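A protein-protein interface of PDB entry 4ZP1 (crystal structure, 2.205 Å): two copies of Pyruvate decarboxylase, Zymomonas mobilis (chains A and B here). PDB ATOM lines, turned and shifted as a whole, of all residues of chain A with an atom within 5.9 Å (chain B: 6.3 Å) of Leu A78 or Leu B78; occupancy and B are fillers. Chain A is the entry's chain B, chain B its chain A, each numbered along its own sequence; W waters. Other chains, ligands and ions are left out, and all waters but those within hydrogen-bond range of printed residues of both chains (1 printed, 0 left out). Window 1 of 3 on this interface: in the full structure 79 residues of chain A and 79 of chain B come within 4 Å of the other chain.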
ATOM      1  N   THR A  72      -6.526 -11.504   3.725  1.00  0.00           N
ATOM      2  CA  THR A  72      -7.422 -10.389   3.981  1.00  0.00           C
ATOM      3  C   THR A  72      -8.854 -10.895   4.190  1.00  0.00           C
ATOM      4  O   THR A  72      -9.155 -12.068   3.969  1.00  0.00           O
ATOM      5  CB  THR A  72      -7.371  -9.359   2.836  1.00  0.00           C
ATOM      6  OG1 THR A  72      -7.981  -8.139   3.262  1.00  0.00           O
ATOM      7  CG2 THR A  72      -8.070  -9.887   1.591  1.00  0.00           C
ATOM      8  N   SER A  74     -12.609 -12.040   4.161  1.00  0.00           N
ATOM      9  CA  SER A  74     -13.599 -12.612   3.251  1.00  0.00           C
ATOM     10  C   SER A  74     -13.049 -13.171   1.952  1.00  0.00           C
ATOM     11  O   SER A  74     -13.028 -14.384   1.752  1.00  0.00           O
ATOM     12  CB  SER A  74     -14.666 -11.575   2.896  1.00  0.00           C
ATOM     13  OG  SER A  74     -15.432 -11.225   4.023  1.00  0.00           O
ATOM     14  N   VAL A  75     -12.663 -12.277   1.050  1.00  0.00           N
ATOM     15  CA  VAL A  75     -12.236 -12.677  -0.281  1.00  0.00           C
ATOM     16  C   VAL A  75     -10.975 -13.522  -0.196  1.00  0.00           C
ATOM     17  O   VAL A  75     -10.757 -14.417  -1.008  1.00  0.00           O
ATOM     18  CB  VAL A  75     -11.990 -11.458  -1.191  1.00  0.00           C
ATOM     19  CG1 VAL A  75     -13.304 -10.755  -1.485  1.00  0.00           C
ATOM     20  CG2 VAL A  75     -10.998 -10.505  -0.544  1.00  0.00           C
ATOM     21  N   GLY A  76     -10.145 -13.243   0.798  1.00  0.00           N
ATOM     22  CA  GLY A  76      -8.936 -14.024   0.994  1.00  0.00           C
ATOM     23  C   GLY A  76      -9.211 -15.261   1.824  1.00  0.00           C
ATOM     24  O   GLY A  76      -8.918 -16.387   1.415  1.00  0.00           O
ATOM     25  N   ALA A  77      -9.806 -15.042   2.990  1.00  0.00           N
ATOM     26  CA  ALA A  77      -9.998 -16.091   3.978  1.00  0.00           C
ATOM     27  C   ALA A  77     -10.826 -17.282   3.480  1.00  0.00           C
ATOM     28  O   ALA A  77     -10.467 -18.428   3.745  1.00  0.00           O
ATOM     29  CB  ALA A  77     -10.632 -15.504   5.222  1.00  0.00           C
ATOM     30  N   LEU A  78     -11.921 -17.024   2.763  1.00  0.00           N
ATOM     31  CA  LEU A  78     -12.839 -18.107   2.410  1.00  0.00           C
ATOM     32  C   LEU A  78     -12.176 -19.166   1.531  1.00  0.00           C
ATOM     33  O   LEU A  78     -12.410 -20.361   1.716  1.00  0.00           O
ATOM     34  CB  LEU A  78     -14.102 -17.564   1.721  1.00  0.00           C
ATOM     35  CG  LEU A  78     -15.331 -17.474   2.636  1.00  0.00           C
ATOM     36  CD1 LEU A  78     -14.995 -16.738   3.922  1.00  0.00           C
ATOM     37  CD2 LEU A  78     -16.507 -16.794   1.953  1.00  0.00           C
ATOM     38  N   SER A  79     -11.351 -18.738   0.580  1.00  0.00           N
ATOM     39  CA  SER A  79     -10.664 -19.691  -0.289  1.00  0.00           C
ATOM     40  C   SER A  79      -9.534 -20.400   0.466  1.00  0.00           C
ATOM     41  O   SER A  79      -9.209 -21.547   0.164  1.00  0.00           O
ATOM     42  CB  SER A  79     -10.116 -18.995  -1.537  1.00  0.00           C
ATOM     43  OG  SER A  79      -9.291 -17.903  -1.174  1.00  0.00           O
ATOM     44  N   ALA A  80      -8.952 -19.723   1.453  1.00  0.00           N
ATOM     45  CA  ALA A  80      -7.897 -20.332   2.268  1.00  0.00           C
ATOM     46  C   ALA A  80      -8.471 -21.362   3.248  1.00  0.00           C
ATOM     47  O   ALA A  80      -7.743 -22.237   3.717  1.00  0.00           O
ATOM     48  CB  ALA A  80      -7.116 -19.260   3.027  1.00  0.00           C
ATOM     49  N   PHE A  81      -9.773 -21.259   3.544  1.00  0.00           N
ATOM     50  CA  PHE A  81     -10.445 -22.213   4.432  1.00  0.00           C
ATOM     51  C   PHE A  81     -10.264 -23.643   3.945  1.00  0.00           C
ATOM     52  O   PHE A  81     -10.163 -24.576   4.740  1.00  0.00           O
ATOM     53  CB  PHE A  81     -11.946 -21.914   4.543  1.00  0.00           C
ATOM     54  CG  PHE A  81     -12.283 -20.825   5.514  1.00  0.00           C
ATOM     55  CD1 PHE A  81     -11.310 -20.291   6.341  1.00  0.00           C
ATOM     56  CD2 PHE A  81     -13.579 -20.342   5.602  1.00  0.00           C
ATOM     57  CE1 PHE A  81     -11.619 -19.287   7.241  1.00  0.00           C
ATOM     58  CE2 PHE A  81     -13.903 -19.337   6.494  1.00  0.00           C
ATOM     59  CZ  PHE A  81     -12.927 -18.806   7.317  1.00  0.00           C
ATOM     60  N   ASP A  82     -10.265 -23.800   2.630  1.00  0.00           N
ATOM     61  CA  ASP A  82     -10.015 -25.086   2.000  1.00  0.00           C
ATOM     62  C   ASP A  82      -8.643 -25.660   2.413  1.00  0.00           C
ATOM     63  O   ASP A  82      -8.514 -26.854   2.700  1.00  0.00           O
ATOM     64  CB  ASP A  82     -10.098 -24.933   0.484  1.00  0.00           C
ATOM     65  CG  ASP A  82     -10.259 -26.254  -0.231  1.00  0.00           C
ATOM     66  OD1 ASP A  82     -10.006 -27.306   0.391  1.00  0.00           O
ATOM     67  OD2 ASP A  82     -10.631 -26.237  -1.424  1.00  0.00           O
ATOM     68  N   GLY A  85      -8.851 -26.529   6.239  1.00  0.00           N
ATOM     69  CA  GLY A  85      -9.498 -27.816   6.392  1.00  0.00           C
ATOM     70  C   GLY A  85      -8.523 -28.957   6.133  1.00  0.00           C
ATOM     71  O   GLY A  85      -8.503 -29.960   6.855  1.00  0.00           O
ATOM     72  N   TYR A 123     -19.589 -13.869  10.263  1.00  0.00           N
ATOM     73  CA  TYR A 123     -19.828 -15.077   9.476  1.00  0.00           C
ATOM     74  C   TYR A 123     -18.528 -15.811   9.146  1.00  0.00           C
ATOM     75  O   TYR A 123     -18.496 -17.035   9.175  1.00  0.00           O
ATOM     76  CB  TYR A 123     -20.598 -14.777   8.187  1.00  0.00           C
ATOM     77  CG  TYR A 123     -19.872 -13.940   7.154  1.00  0.00           C
ATOM     78  CD1 TYR A 123     -19.045 -14.524   6.197  1.00  0.00           C
ATOM     79  CD2 TYR A 123     -20.054 -12.564   7.106  1.00  0.00           C
ATOM     80  CE1 TYR A 123     -18.395 -13.747   5.239  1.00  0.00           C
ATOM     81  CE2 TYR A 123     -19.415 -11.783   6.157  1.00  0.00           C
ATOM     82  CZ  TYR A 123     -18.590 -12.375   5.232  1.00  0.00           C
ATOM     83  OH  TYR A 123     -17.973 -11.570   4.297  1.00  0.00           O
ATOM     84  N   GLN A 124     -17.473 -15.068   8.833  1.00  0.00           N
ATOM     85  CA  GLN A 124     -16.187 -15.680   8.547  1.00  0.00           C
ATOM     86  C   GLN A 124     -15.711 -16.468   9.763  1.00  0.00           C
ATOM     87  O   GLN A 124     -15.350 -17.640   9.648  1.00  0.00           O
ATOM     88  CB  GLN A 124     -15.149 -14.632   8.142  1.00  0.00           C
ATOM     89  CG  GLN A 124     -13.767 -15.222   7.902  1.00  0.00           C
ATOM     90  CD  GLN A 124     -12.804 -14.228   7.279  1.00  0.00           C
ATOM     91  OE1 GLN A 124     -13.044 -13.724   6.179  1.00  0.00           O
ATOM     92  NE2 GLN A 124     -11.704 -13.943   7.980  1.00  0.00           N
ATOM     93  N   MET A 127     -17.842 -19.580  10.250  1.00  0.00           N
ATOM     94  CA  MET A 127     -17.443 -20.624   9.321  1.00  0.00           C
ATOM     95  C   MET A 127     -16.131 -21.268   9.787  1.00  0.00           C
ATOM     96  O   MET A 127     -16.020 -22.492   9.833  1.00  0.00           O
ATOM     97  CB  MET A 127     -17.310 -20.058   7.904  1.00  0.00           C
ATOM     98  CG  MET A 127     -18.648 -19.520   7.335  1.00  0.00           C
ATOM     99  SD  MET A 127     -18.424 -18.700   5.742  1.00  0.00           S
ATOM    100  CE  MET A 127     -18.118 -20.101   4.668  1.00  0.00           C
ATOM    101  N   ILE A 131     -13.689 -25.819  11.185  1.00  0.00           N
ATOM    102  CA  ILE A 131     -12.534 -26.449  10.567  1.00  0.00           C
ATOM    103  C   ILE A 131     -11.232 -26.105  11.287  1.00  0.00           C
ATOM    104  O   ILE A 131     -10.162 -26.151  10.702  1.00  0.00           O
ATOM    105  CB  ILE A 131     -12.431 -26.045   9.090  1.00  0.00           C
ATOM    106  CG1 ILE A 131     -12.311 -24.526   8.967  1.00  0.00           C
ATOM    107  CG2 ILE A 131     -13.658 -26.529   8.328  1.00  0.00           C
ATOM    108  CD1 ILE A 131     -12.106 -24.052   7.551  1.00  0.00           C
ATOM    109  N   TRP A 412      -7.033 -35.594   3.301  1.00  0.00           N
ATOM    110  CA  TRP A 412      -7.732 -34.494   2.640  1.00  0.00           C
ATOM    111  C   TRP A 412      -7.837 -34.756   1.145  1.00  0.00           C
ATOM    112  O   TRP A 412      -8.917 -34.689   0.587  1.00  0.00           O
ATOM    113  CB  TRP A 412      -7.030 -33.163   2.898  1.00  0.00           C
ATOM    114  CG  TRP A 412      -7.889 -31.934   2.655  1.00  0.00           C
ATOM    115  CD1 TRP A 412      -7.600 -30.878   1.831  1.00  0.00           C
ATOM    116  CD2 TRP A 412      -9.154 -31.628   3.264  1.00  0.00           C
ATOM    117  NE1 TRP A 412      -8.606 -29.944   1.884  1.00  0.00           N
ATOM    118  CE2 TRP A 412      -9.572 -30.377   2.755  1.00  0.00           C
ATOM    119  CE3 TRP A 412      -9.977 -32.290   4.184  1.00  0.00           C
ATOM    120  CZ2 TRP A 412     -10.773 -29.775   3.138  1.00  0.00           C
ATOM    121  CZ3 TRP A 412     -11.178 -31.686   4.561  1.00  0.00           C
ATOM    122  CH2 TRP A 412     -11.557 -30.445   4.041  1.00  0.00           C
ATOM    123  N   VAL B  71     -19.490 -29.202  -7.868  1.00  0.00           N
ATOM    124  CA  VAL B  71     -18.183 -29.528  -7.315  1.00  0.00           C
ATOM    125  C   VAL B  71     -18.266 -30.816  -6.495  1.00  0.00           C
ATOM    126  O   VAL B  71     -19.331 -31.417  -6.383  1.00  0.00           O
ATOM    127  CB  VAL B  71     -17.642 -28.374  -6.444  1.00  0.00           C
ATOM    128  CG1 VAL B  71     -17.522 -27.099  -7.273  1.00  0.00           C
ATOM    129  CG2 VAL B  71     -18.551 -28.143  -5.247  1.00  0.00           C
ATOM    130  N   THR B  72     -17.144 -31.256  -5.939  1.00  0.00           N
ATOM    131  CA  THR B  72     -17.172 -32.470  -5.141  1.00  0.00           C
ATOM    132  C   THR B  72     -17.200 -32.107  -3.658  1.00  0.00           C
ATOM    133  O   THR B  72     -17.018 -30.948  -3.290  1.00  0.00           O
ATOM    134  CB  THR B  72     -15.974 -33.398  -5.461  1.00  0.00           C
ATOM    135  OG1 THR B  72     -16.224 -34.703  -4.926  1.00  0.00           O
ATOM    136  CG2 THR B  72     -14.669 -32.847  -4.893  1.00  0.00           C
ATOM    137  N   SER B  74     -16.417 -31.250   0.004  1.00  0.00           N
ATOM    138  CA  SER B  74     -15.378 -30.783   0.919  1.00  0.00           C
ATOM    139  C   SER B  74     -14.182 -30.105   0.238  1.00  0.00           C
ATOM    140  O   SER B  74     -14.040 -28.883   0.311  1.00  0.00           O
ATOM    141  CB  SER B  74     -14.894 -31.952   1.780  1.00  0.00           C
ATOM    142  OG  SER B  74     -14.090 -31.501   2.855  1.00  0.00           O
ATOM    143  N   VAL B  75     -13.307 -30.884  -0.392  1.00  0.00           N
ATOM    144  CA  VAL B  75     -12.147 -30.299  -1.069  1.00  0.00           C
ATOM    145  C   VAL B  75     -12.587 -29.430  -2.253  1.00  0.00           C
ATOM    146  O   VAL B  75     -11.939 -28.436  -2.598  1.00  0.00           O
ATOM    147  CB  VAL B  75     -11.153 -31.382  -1.566  1.00  0.00           C
ATOM    148  CG1 VAL B  75     -10.471 -32.073  -0.383  1.00  0.00           C
ATOM    149  CG2 VAL B  75     -11.855 -32.395  -2.478  1.00  0.00           C
ATOM    150  N   GLY B  76     -13.704 -29.798  -2.866  1.00  0.00           N
ATOM    151  CA  GLY B  76     -14.234 -29.021  -3.971  1.00  0.00           C
ATOM    152  C   GLY B  76     -14.969 -27.788  -3.484  1.00  0.00           C
ATOM    153  O   GLY B  76     -14.688 -26.665  -3.911  1.00  0.00           O
ATOM    154  N   ALA B  77     -15.898 -28.001  -2.559  1.00  0.00           N
ATOM    155  CA  ALA B  77     -16.840 -26.961  -2.173  1.00  0.00           C
ATOM    156  C   ALA B  77     -16.207 -25.797  -1.401  1.00  0.00           C
ATOM    157  O   ALA B  77     -16.606 -24.647  -1.577  1.00  0.00           O
ATOM    158  CB  ALA B  77     -17.972 -27.575  -1.358  1.00  0.00           C
ATOM    159  N   LEU B  78     -15.220 -26.080  -0.558  1.00  0.00           N
ATOM    160  CA  LEU B  78     -14.715 -25.047   0.333  1.00  0.00           C
ATOM    161  C   LEU B  78     -14.096 -23.876  -0.423  1.00  0.00           C
ATOM    162  O   LEU B  78     -14.301 -22.722  -0.038  1.00  0.00           O
ATOM    163  CB  LEU B  78     -13.714 -25.634   1.329  1.00  0.00           C
ATOM    164  CG  LEU B  78     -14.354 -25.926   2.690  1.00  0.00           C
ATOM    165  CD1 LEU B  78     -15.652 -26.698   2.496  1.00  0.00           C
ATOM    166  CD2 LEU B  78     -13.411 -26.686   3.617  1.00  0.00           C
ATOM    167  N   SER B  79     -13.363 -24.145  -1.500  1.00  0.00           N
ATOM    168  CA  SER B  79     -12.800 -23.044  -2.277  1.00  0.00           C
ATOM    169  C   SER B  79     -13.886 -22.357  -3.115  1.00  0.00           C
ATOM    170  O   SER B  79     -13.811 -21.155  -3.375  1.00  0.00           O
ATOM    171  CB  SER B  79     -11.649 -23.524  -3.165  1.00  0.00           C
ATOM    172  OG  SER B  79     -12.007 -24.679  -3.899  1.00  0.00           O
ATOM    173  N   ALA B  80     -14.907 -23.117  -3.505  1.00  0.00           N
ATOM    174  CA  ALA B  80     -16.020 -22.577  -4.273  1.00  0.00           C
ATOM    175  C   ALA B  80     -16.831 -21.572  -3.446  1.00  0.00           C
ATOM    176  O   ALA B  80     -17.420 -20.649  -4.000  1.00  0.00           O
ATOM    177  CB  ALA B  80     -16.903 -23.693  -4.762  1.00  0.00           C
ATOM    178  N   PHE B  81     -16.838 -21.749  -2.124  1.00  0.00           N
ATOM    179  CA  PHE B  81     -17.579 -20.867  -1.224  1.00  0.00           C
ATOM    180  C   PHE B  81     -17.197 -19.405  -1.401  1.00  0.00           C
ATOM    181  O   PHE B  81     -18.017 -18.510  -1.217  1.00  0.00           O
ATOM    182  CB  PHE B  81     -17.354 -21.272   0.236  1.00  0.00           C
ATOM    183  CG  PHE B  81     -18.175 -22.461   0.674  1.00  0.00           C
ATOM    184  CD1 PHE B  81     -18.046 -22.973   1.958  1.00  0.00           C
ATOM    185  CD2 PHE B  81     -19.063 -23.068  -0.196  1.00  0.00           C
ATOM    186  CE1 PHE B  81     -18.795 -24.062   2.366  1.00  0.00           C
ATOM    187  CE2 PHE B  81     -19.814 -24.161   0.203  1.00  0.00           C
ATOM    188  CZ  PHE B  81     -19.683 -24.657   1.485  1.00  0.00           C
ATOM    189  N   ASP B  82     -15.936 -19.170  -1.739  1.00  0.00           N
ATOM    190  CA  ASP B  82     -15.440 -17.827  -1.997  1.00  0.00           C
ATOM    191  C   ASP B  82     -16.181 -17.217  -3.182  1.00  0.00           C
ATOM    192  O   ASP B  82     -16.519 -16.032  -3.184  1.00  0.00           O
ATOM    193  CB  ASP B  82     -13.940 -17.867  -2.272  1.00  0.00           C
ATOM    194  CG  ASP B  82     -13.261 -16.542  -2.015  1.00  0.00           C
ATOM    195  OD1 ASP B  82     -13.941 -15.495  -1.987  1.00  0.00           O
ATOM    196  OD2 ASP B  82     -12.028 -16.553  -1.845  1.00  0.00           O
ATOM    197  N   ALA B  83     -16.430 -18.040  -4.194  1.00  0.00           N
ATOM    198  CA  ALA B  83     -17.137 -17.593  -5.379  1.00  0.00           C
ATOM    199  C   ALA B  83     -18.617 -17.420  -5.053  1.00  0.00           C
ATOM    200  O   ALA B  83     -19.266 -16.482  -5.519  1.00  0.00           O
ATOM    201  CB  ALA B  83     -16.948 -18.575  -6.510  1.00  0.00           C
ATOM    202  N   GLY B  85     -19.846 -16.735  -2.085  1.00  0.00           N
ATOM    203  CA  GLY B  85     -19.900 -15.506  -1.322  1.00  0.00           C
ATOM    204  C   GLY B  85     -19.978 -14.311  -2.259  1.00  0.00           C
ATOM    205  O   GLY B  85     -20.763 -13.386  -2.042  1.00  0.00           O
ATOM    206  N   LEU B 116     -12.697 -34.070   7.297  1.00  0.00           N
ATOM    207  CA  LEU B 116     -11.825 -33.546   8.339  1.00  0.00           C
ATOM    208  C   LEU B 116     -11.166 -34.618   9.206  1.00  0.00           C
ATOM    209  O   LEU B 116     -10.228 -34.331   9.938  1.00  0.00           O
ATOM    210  CB  LEU B 116     -12.608 -32.583   9.232  1.00  0.00           C
ATOM    211  CG  LEU B 116     -13.055 -31.253   8.621  1.00  0.00           C
ATOM    212  CD1 LEU B 116     -14.041 -30.575   9.563  1.00  0.00           C
ATOM    213  CD2 LEU B 116     -11.856 -30.343   8.358  1.00  0.00           C
ATOM    214  N   TYR B 123     -20.693 -30.194   8.597  1.00  0.00           N
ATOM    215  CA  TYR B 123     -19.956 -28.931   8.734  1.00  0.00           C
ATOM    216  C   TYR B 123     -19.967 -28.108   7.450  1.00  0.00           C
ATOM    217  O   TYR B 123     -19.979 -26.882   7.504  1.00  0.00           O
ATOM    218  CB  TYR B 123     -18.501 -29.167   9.162  1.00  0.00           C
ATOM    219  CG  TYR B 123     -17.648 -29.861   8.128  1.00  0.00           C
ATOM    220  CD1 TYR B 123     -17.554 -31.242   8.108  1.00  0.00           C
ATOM    221  CD2 TYR B 123     -16.933 -29.140   7.175  1.00  0.00           C
ATOM    222  CE1 TYR B 123     -16.780 -31.895   7.176  1.00  0.00           C
ATOM    223  CE2 TYR B 123     -16.148 -29.791   6.228  1.00  0.00           C
ATOM    224  CZ  TYR B 123     -16.076 -31.174   6.241  1.00  0.00           C
ATOM    225  OH  TYR B 123     -15.307 -31.865   5.324  1.00  0.00           O
ATOM    226  N   GLN B 124     -19.936 -28.773   6.301  1.00  0.00           N
ATOM    227  CA  GLN B 124     -19.962 -28.068   5.021  1.00  0.00           C
ATOM    228  C   GLN B 124     -21.315 -27.383   4.798  1.00  0.00           C
ATOM    229  O   GLN B 124     -21.384 -26.254   4.305  1.00  0.00           O
ATOM    230  CB  GLN B 124     -19.656 -29.027   3.863  1.00  0.00           C
ATOM    231  CG  GLN B 124     -19.692 -28.347   2.500  1.00  0.00           C
ATOM    232  CD  GLN B 124     -19.192 -29.240   1.386  1.00  0.00           C
ATOM    233  OE1 GLN B 124     -18.157 -29.890   1.516  1.00  0.00           O
ATOM    234  NE2 GLN B 124     -19.933 -29.287   0.282  1.00  0.00           N
ATOM    235  N   MET B 127     -21.456 -24.396   7.028  1.00  0.00           N
ATOM    236  CA  MET B 127     -20.656 -23.275   6.531  1.00  0.00           C
ATOM    237  C   MET B 127     -21.439 -22.544   5.444  1.00  0.00           C
ATOM    238  O   MET B 127     -21.569 -21.319   5.474  1.00  0.00           O
ATOM    239  CB  MET B 127     -19.293 -23.745   6.006  1.00  0.00           C
ATOM    240  CG  MET B 127     -18.337 -24.212   7.103  1.00  0.00           C
ATOM    241  SD  MET B 127     -16.834 -25.004   6.479  1.00  0.00           S
ATOM    242  CE  MET B 127     -15.858 -23.576   5.994  1.00  0.00           C
ATOM    243  N   ILE B 131     -23.497 -18.027   3.718  1.00  0.00           N
ATOM    244  CA  ILE B 131     -23.229 -17.290   2.483  1.00  0.00           C
ATOM    245  C   ILE B 131     -24.193 -17.627   1.343  1.00  0.00           C
ATOM    246  O   ILE B 131     -23.859 -17.420   0.176  1.00  0.00           O
ATOM    247  CB  ILE B 131     -21.795 -17.561   1.986  1.00  0.00           C
ATOM    248  CG1 ILE B 131     -21.607 -19.057   1.740  1.00  0.00           C
ATOM    249  CG2 ILE B 131     -20.755 -17.050   2.994  1.00  0.00           C
ATOM    250  CD1 ILE B 131     -20.261 -19.408   1.152  1.00  0.00           C
ATOM    251  N   TRP B 412     -17.930  -7.437  -3.791  1.00  0.00           N
ATOM    252  CA  TRP B 412     -17.097  -8.533  -3.320  1.00  0.00           C
ATOM    253  C   TRP B 412     -15.618  -8.167  -3.478  1.00  0.00           C
ATOM    254  O   TRP B 412     -14.833  -8.276  -2.540  1.00  0.00           O
ATOM    255  CB  TRP B 412     -17.433  -9.809  -4.086  1.00  0.00           C
ATOM    256  CG  TRP B 412     -16.924 -11.064  -3.449  1.00  0.00           C
ATOM    257  CD1 TRP B 412     -16.138 -12.021  -4.032  1.00  0.00           C
ATOM    258  CD2 TRP B 412     -17.176 -11.515  -2.110  1.00  0.00           C
ATOM    259  NE1 TRP B 412     -15.885 -13.038  -3.137  1.00  0.00           N
ATOM    260  CE2 TRP B 412     -16.505 -12.748  -1.949  1.00  0.00           C
ATOM    261  CE3 TRP B 412     -17.893 -10.993  -1.031  1.00  0.00           C
ATOM    262  CZ2 TRP B 412     -16.538 -13.466  -0.755  1.00  0.00           C
ATOM    263  CZ3 TRP B 412     -17.925 -11.709   0.155  1.00  0.00           C
ATOM    264  CH2 TRP B 412     -17.252 -12.934   0.282  1.00  0.00           C
HETATM  265  O   HOH W   1     -14.698 -21.915   2.684  1.00  0.00           O
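OE1 of Gln B124 sits at hydrogen-bond distance from N of Ser B74 (2.7 Å). O of Gly A76 is in hydrogen-bond range of OG of Ser A79, 3.0 Å away. The backbone carbonyl oxygen (O) of Asp B82 sits at hydrogen-bond distance from the indole nitrogen (NE1) of Trp B412. OE1 of Gln A124 lies within hydrogen-bond range of N of Ser A74, at 2.7 Å. OG of Ser B79 sits at hydrogen-bond distance from O of Gly B76. The side-chain hydroxyl (OH) of Tyr B123 lies within hydrogen-bond range of the side-chain hydroxyl (OG) of Ser B74.
Of the 16 printed residues of chain A, 10 touch a printed residue of chain B. Printed residues of chain A that touch a printed residue of chain B: Ser A74, Val A75, Leu A78, Ser A79, Phe A81, Asp A82, Gly A85, Met A127, Ile A131 and Trp A412. Hydrophobic or aromatic side chains of chain A within 4 Å of the printed part of chain B: Val A75, Leu A78, Phe A81, Met A127, Ile A131 and Trp A412. Along chain A the printed residues that touch a printed residue of chain B span positions 74 to 412. Printed residues of chain B that touch a printed residue of chain A: Ser B74, Val B75, Leu B78, Ser B79, Phe B81, Asp B82, Leu B116, Met B127, Ile B131 and Trp B412. Hydrophobic or aromatic side chains of chain B within 4 Å of the printed part of chain A: Val B75, Leu B78, Phe B81, Leu B116, Met B127, Ile B131 and Trp B412. Among the printed residues, 19 pairs touch across the chains.
Val A75 touches Trp B412, and with the chains exchanged Trp A412 touches Val B75. Leu B78 touches its own counterpart, Leu A78. Met A127 touches its own counterpart, Met B127. Met A127 touches Ile B131, and with the chains exchanged Ile A131 touches Met B127. Of the 19 pairs that touch across the chains among the printed residues, 16 have their exchanged pair printed and touching as well.
The backbone carbonyl oxygen of Leu B78 lies close to the backbone carbonyl oxygen of Leu A78, 3.5 Å away. O of Val A75 sits close to OD2 of Asp B82 (2.6 Å). OD2 of Asp A82 lies close to O of Val B75, 2.8 Å away. The side-chain hydroxyl (OG) of Ser A79 lies close to the side-chain carboxylate (OD2) of Asp B82 (3.1 Å). OG of Ser B79 is in hydrogen-bond range of OD2 of Asp A82 (3.2 Å).
Of the printed residues of chain B, Ser A74 touches Trp B412. Leu A78 touches just these residues of chain B: Leu B78, Phe B81 and Asp B82. Of the printed residues of chain B, Met A127 touches Phe B81 (3.9 Å), Met B127 (3.7 Å) and Ile B131 (3.96 Å). Leu B78 touches two residues of chain A. Of the printed residues of chain A, Ser B79 touches Asp A82. The nearest residue of chain B that does not touch Leu A78 is Trp B412 (4.3 Å). The nearest residue of chain A that does not touch Leu B78 is Phe A81 (4.03 Å).
Ser A74 touches Trp B412 (CB to CH2, 3.9 Å). O of Trp B412 touches CG1 of Val A75, at 3.1 Å. Leu A78 touches Phe B81 (CD2 to O, 3.9 Å). CB of Leu A78 touches CA of Asp B82 (3.96 Å). Phe A81 touches Met B127. Asp A82 touches Leu B78. Met A127 touches Met B127 (CE to O, 3.7 Å). Ile A131 touches Met B127 (CG2 to SD, 3.98 Å). OG of Ser B74 touches CH2 of Trp A412, at 3.0 Å. Trp A412 touches Val B75.
Water W1 bridges O of Leu B78 (2.9 Å) and O of Leu A78 (2.9 Å).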
